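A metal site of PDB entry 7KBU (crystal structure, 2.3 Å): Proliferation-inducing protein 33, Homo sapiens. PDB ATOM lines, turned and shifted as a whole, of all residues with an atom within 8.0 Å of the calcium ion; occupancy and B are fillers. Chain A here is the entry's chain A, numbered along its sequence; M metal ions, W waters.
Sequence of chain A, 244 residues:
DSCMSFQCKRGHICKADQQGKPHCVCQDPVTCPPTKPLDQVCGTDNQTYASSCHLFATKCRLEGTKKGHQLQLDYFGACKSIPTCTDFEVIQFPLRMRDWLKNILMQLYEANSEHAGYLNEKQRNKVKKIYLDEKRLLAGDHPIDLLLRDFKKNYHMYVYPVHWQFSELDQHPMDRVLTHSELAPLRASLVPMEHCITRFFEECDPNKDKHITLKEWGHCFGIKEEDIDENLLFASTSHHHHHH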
ATOM      1  N   PHE A 166     -16.631 -33.029   9.720  1.00  0.00           N
ATOM      2  CA  PHE A 166     -17.532 -32.262   8.866  1.00  0.00           C
ATOM      3  C   PHE A 166     -18.873 -32.965   8.724  1.00  0.00           C
ATOM      4  O   PHE A 166     -19.929 -32.376   8.947  1.00  0.00           O
ATOM      5  CB  PHE A 166     -16.867 -32.053   7.501  1.00  0.00           C
ATOM      6  CG  PHE A 166     -17.662 -31.195   6.517  1.00  0.00           C
ATOM      7  CD1 PHE A 166     -18.690 -31.741   5.765  1.00  0.00           C
ATOM      8  CD2 PHE A 166     -17.326 -29.870   6.313  1.00  0.00           C
ATOM      9  CE1 PHE A 166     -19.397 -30.959   4.838  1.00  0.00           C
ATOM     10  CE2 PHE A 166     -18.024 -29.086   5.396  1.00  0.00           C
ATOM     11  CZ  PHE A 166     -19.053 -29.634   4.654  1.00  0.00           C
ATOM     12  N   LEU A 169     -21.197 -32.858  11.581  1.00  0.00           N
ATOM     13  CA  LEU A 169     -21.859 -31.574  11.836  1.00  0.00           C
ATOM     14  C   LEU A 169     -22.856 -31.207  10.743  1.00  0.00           C
ATOM     15  O   LEU A 169     -23.785 -30.428  11.024  1.00  0.00           O
ATOM     16  CB  LEU A 169     -20.814 -30.454  11.964  1.00  0.00           C
ATOM     17  CG  LEU A 169     -19.807 -30.626  13.116  1.00  0.00           C
ATOM     18  CD1 LEU A 169     -18.667 -29.658  13.007  1.00  0.00           C
ATOM     19  CD2 LEU A 169     -20.469 -30.461  14.445  1.00  0.00           C
ATOM     20  N   ASP A 170     -22.731 -31.781   9.544  1.00  0.00           N
ATOM     21  CA  ASP A 170     -23.537 -31.359   8.394  1.00  0.00           C
ATOM     22  C   ASP A 170     -24.843 -32.144   8.405  1.00  0.00           C
ATOM     23  O   ASP A 170     -25.091 -33.046   7.594  1.00  0.00           O
ATOM     24  CB  ASP A 170     -22.764 -31.557   7.100  1.00  0.00           C
ATOM     25  CG  ASP A 170     -23.584 -31.161   5.864  1.00  0.00           C
ATOM     26  OD1 ASP A 170     -24.284 -30.140   5.935  1.00  0.00           O
ATOM     27  OD2 ASP A 170     -23.481 -31.832   4.811  1.00  0.00           O
ATOM     28  N   GLN A 171     -25.730 -31.744   9.314  1.00  0.00           N
ATOM     29  CA  GLN A 171     -26.969 -32.465   9.563  1.00  0.00           C
ATOM     30  C   GLN A 171     -28.228 -31.613   9.635  1.00  0.00           C
ATOM     31  O   GLN A 171     -29.310 -32.179   9.697  1.00  0.00           O
ATOM     32  CB  GLN A 171     -26.854 -33.253  10.887  1.00  0.00           C
ATOM     33  CG  GLN A 171     -25.682 -34.220  10.943  1.00  0.00           C
ATOM     34  CD  GLN A 171     -25.866 -35.463  10.067  1.00  0.00           C
ATOM     35  OE1 GLN A 171     -26.989 -35.914   9.858  1.00  0.00           O
ATOM     36  NE2 GLN A 171     -24.765 -36.015   9.559  1.00  0.00           N
ATOM     37  N   HIS A 172     -28.138 -30.280   9.624  1.00  0.00           N
ATOM     38  CA  HIS A 172     -29.283 -29.424   9.940  1.00  0.00           C
ATOM     39  C   HIS A 172     -29.328 -28.239   8.994  1.00  0.00           C
ATOM     40  O   HIS A 172     -29.198 -27.084   9.416  1.00  0.00           O
ATOM     41  CB  HIS A 172     -29.228 -28.963  11.390  1.00  0.00           C
ATOM     42  CG  HIS A 172     -29.156 -30.082  12.388  1.00  0.00           C
ATOM     43  ND1 HIS A 172     -28.026 -30.356  13.121  1.00  0.00           N
ATOM     44  CD2 HIS A 172     -30.080 -31.007  12.766  1.00  0.00           C
ATOM     45  CE1 HIS A 172     -28.244 -31.401  13.913  1.00  0.00           C
ATOM     46  NE2 HIS A 172     -29.486 -31.805  13.712  1.00  0.00           N
ATOM     47  N   PRO A 173     -29.539 -28.470   7.685  1.00  0.00           N
ATOM     48  CA  PRO A 173     -29.712 -29.780   7.044  1.00  0.00           C
ATOM     49  C   PRO A 173     -28.423 -30.330   6.461  1.00  0.00           C
ATOM     50  O   PRO A 173     -27.444 -29.596   6.324  1.00  0.00           O
ATOM     51  CB  PRO A 173     -30.706 -29.482   5.921  1.00  0.00           C
ATOM     52  CG  PRO A 173     -30.441 -28.022   5.558  1.00  0.00           C
ATOM     53  CD  PRO A 173     -29.668 -27.381   6.708  1.00  0.00           C
ATOM     54  N   MET A 174     -28.429 -31.598   6.062  1.00  0.00           N
ATOM     55  CA  MET A 174     -27.283 -32.201   5.398  1.00  0.00           C
ATOM     56  C   MET A 174     -27.270 -31.727   3.948  1.00  0.00           C
ATOM     57  O   MET A 174     -28.152 -32.077   3.165  1.00  0.00           O
ATOM     58  CB  MET A 174     -27.329 -33.719   5.487  1.00  0.00           C
ATOM     59  CG  MET A 174     -26.193 -34.388   4.722  1.00  0.00           C
ATOM     60  SD  MET A 174     -26.389 -36.167   4.507  1.00  0.00           S
ATOM     61  CE  MET A 174     -26.537 -36.741   6.185  1.00  0.00           C
ATOM     62  N   ASP A 175     -26.252 -30.924   3.591  1.00  0.00           N
ATOM     63  CA  ASP A 175     -26.221 -30.341   2.249  1.00  0.00           C
ATOM     64  C   ASP A 175     -24.804 -30.048   1.800  1.00  0.00           C
ATOM     65  O   ASP A 175     -24.624 -29.249   0.867  1.00  0.00           O
ATOM     66  CB  ASP A 175     -27.046 -29.048   2.188  1.00  0.00           C
ATOM     67  CG  ASP A 175     -26.593 -28.004   3.209  1.00  0.00           C
ATOM     68  OD1 ASP A 175     -25.551 -28.188   3.856  1.00  0.00           O
ATOM     69  OD2 ASP A 175     -27.289 -26.977   3.322  1.00  0.00           O
ATOM     70  N   ARG A 176     -23.797 -30.650   2.423  1.00  0.00           N
ATOM     71  CA  ARG A 176     -22.403 -30.517   2.030  1.00  0.00           C
ATOM     72  C   ARG A 176     -21.841 -29.129   2.309  1.00  0.00           C
ATOM     73  O   ARG A 176     -20.772 -28.766   1.801  1.00  0.00           O
ATOM     74  CB  ARG A 176     -22.238 -30.886   0.539  1.00  0.00           C
ATOM     75  CG  ARG A 176     -21.778 -32.318   0.317  1.00  0.00           C
ATOM     76  CD  ARG A 176     -22.931 -33.327   0.207  1.00  0.00           C
ATOM     77  NE  ARG A 176     -22.454 -34.712   0.246  1.00  0.00           N
ATOM     78  CZ  ARG A 176     -22.095 -35.432  -0.813  1.00  0.00           C
ATOM     79  NH1 ARG A 176     -22.159 -34.934  -2.043  1.00  0.00           N
ATOM     80  NH2 ARG A 176     -21.655 -36.677  -0.635  1.00  0.00           N
ATOM     81  N   VAL A 177     -22.509 -28.328   3.142  1.00  0.00           N
ATOM     82  CA  VAL A 177     -21.943 -27.095   3.663  1.00  0.00           C
ATOM     83  C   VAL A 177     -22.343 -26.994   5.125  1.00  0.00           C
ATOM     84  O   VAL A 177     -23.366 -27.554   5.547  1.00  0.00           O
ATOM     85  CB  VAL A 177     -22.405 -25.818   2.909  1.00  0.00           C
ATOM     86  CG1 VAL A 177     -22.301 -26.003   1.400  1.00  0.00           C
ATOM     87  CG2 VAL A 177     -23.821 -25.429   3.286  1.00  0.00           C
ATOM     88  N   LEU A 178     -21.507 -26.299   5.903  1.00  0.00           N
ATOM     89  CA  LEU A 178     -21.770 -26.022   7.301  1.00  0.00           C
ATOM     90  C   LEU A 178     -22.161 -24.553   7.474  1.00  0.00           C
ATOM     91  O   LEU A 178     -21.555 -23.664   6.863  1.00  0.00           O
ATOM     92  CB  LEU A 178     -20.536 -26.310   8.151  1.00  0.00           C
ATOM     93  CG  LEU A 178     -19.930 -27.725   8.065  1.00  0.00           C
ATOM     94  CD1 LEU A 178     -18.695 -27.790   8.988  1.00  0.00           C
ATOM     95  CD2 LEU A 178     -20.936 -28.801   8.444  1.00  0.00           C
ATOM     96  N   THR A 179     -23.182 -24.309   8.298  1.00  0.00           N
ATOM     97  CA  THR A 179     -23.604 -22.967   8.672  1.00  0.00           C
ATOM     98  C   THR A 179     -23.369 -22.751  10.163  1.00  0.00           C
ATOM     99  O   THR A 179     -23.019 -23.674  10.919  1.00  0.00           O
ATOM    100  CB  THR A 179     -25.089 -22.738   8.371  1.00  0.00           C
ATOM    101  OG1 THR A 179     -25.871 -23.684   9.101  1.00  0.00           O
ATOM    102  CG2 THR A 179     -25.376 -22.844   6.882  1.00  0.00           C
ATOM    103  N   SER A 181     -25.301 -22.370  12.696  1.00  0.00           N
ATOM    104  CA  SER A 181     -26.073 -23.162  13.653  1.00  0.00           C
ATOM    105  C   SER A 181     -25.567 -24.598  13.748  1.00  0.00           C
ATOM    106  O   SER A 181     -25.695 -25.227  14.802  1.00  0.00           O
ATOM    107  CB  SER A 181     -27.551 -23.143  13.281  1.00  0.00           C
ATOM    108  OG  SER A 181     -27.867 -24.244  12.466  1.00  0.00           O
ATOM    109  N   GLU A 182     -24.954 -25.103  12.680  1.00  0.00           N
ATOM    110  CA  GLU A 182     -24.410 -26.454  12.690  1.00  0.00           C
ATOM    111  C   GLU A 182     -23.093 -26.516  13.448  1.00  0.00           C
ATOM    112  O   GLU A 182     -22.788 -27.550  14.062  1.00  0.00           O
ATOM    113  CB  GLU A 182     -24.202 -26.965  11.263  1.00  0.00           C
ATOM    114  CG  GLU A 182     -25.473 -27.542  10.598  1.00  0.00           C
ATOM    115  CD  GLU A 182     -25.296 -27.844   9.108  1.00  0.00           C
ATOM    116  OE1 GLU A 182     -24.491 -27.123   8.469  1.00  0.00           O
ATOM    117  OE2 GLU A 182     -25.947 -28.775   8.574  1.00  0.00           O
ATOM    118  N   HIS A 211     -21.224 -19.786   4.506  1.00  0.00           N
ATOM    119  CA  HIS A 211     -21.365 -21.214   4.306  1.00  0.00           C
ATOM    120  C   HIS A 211     -19.961 -21.755   4.119  1.00  0.00           C
ATOM    121  O   HIS A 211     -19.189 -21.214   3.318  1.00  0.00           O
ATOM    122  CB  HIS A 211     -22.240 -21.553   3.100  1.00  0.00           C
ATOM    123  CG  HIS A 211     -23.644 -21.056   3.220  1.00  0.00           C
ATOM    124  ND1 HIS A 211     -24.005 -19.768   2.891  1.00  0.00           N
ATOM    125  CD2 HIS A 211     -24.768 -21.668   3.646  1.00  0.00           C
ATOM    126  CE1 HIS A 211     -25.303 -19.608   3.102  1.00  0.00           C
ATOM    127  NE2 HIS A 211     -25.788 -20.747   3.565  1.00  0.00           N
ATOM    128  N   ILE A 212     -19.628 -22.826   4.842  1.00  0.00           N
ATOM    129  CA  ILE A 212     -18.302 -23.438   4.780  1.00  0.00           C
ATOM    130  C   ILE A 212     -18.442 -24.731   4.001  1.00  0.00           C
ATOM    131  O   ILE A 212     -19.120 -25.664   4.448  1.00  0.00           O
ATOM    132  CB  ILE A 212     -17.736 -23.678   6.180  1.00  0.00           C
ATOM    133  CG1 ILE A 212     -17.474 -22.337   6.874  1.00  0.00           C
ATOM    134  CG2 ILE A 212     -16.441 -24.509   6.114  1.00  0.00           C
ATOM    135  CD1 ILE A 212     -17.251 -22.468   8.334  1.00  0.00           C
HETATM  136 CA    CA M   1     -25.404 -28.261   6.382  1.00  0.00          CA
HETATM  137  O   HOH W   1     -26.424 -26.234   6.118  1.00  0.00           O
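N of Arg 176 lies within hydrogen-bond range of OD2 of Asp 170 (2.7 Å).
N of Thr 179 sits close to OE1 of Glu 182 (3.1 Å).
The side-chain carboxylate of Glu 182 sits close to the backbone NH of Gln 171 (3.1 Å).
OE2 of Glu 182 sits close to N of His 172, at 2.9 Å.
Of the 16 residues printed, 5 come within 4 Å of the calcium ion.
The nearest printed residue that does not touch the calcium ion is Leu 178 (4.4 Å).
The calcium ion is bound by the side-chain carboxylate (OD1) of Asp 170 (2.2 Å), water W1 (2.3 Å), the backbone carbonyl oxygen (O) of Val 177 (2.3 Å), the side-chain carboxylate (OE2) of Glu 182 (2.3 Å), the backbone carbonyl oxygen (O) of Pro 173 (2.4 Å), the side-chain carboxylate (OD1) of Asp 175 (2.5 Å) and the side-chain carboxylate (OE1) of Glu 182 (2.5 Å).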
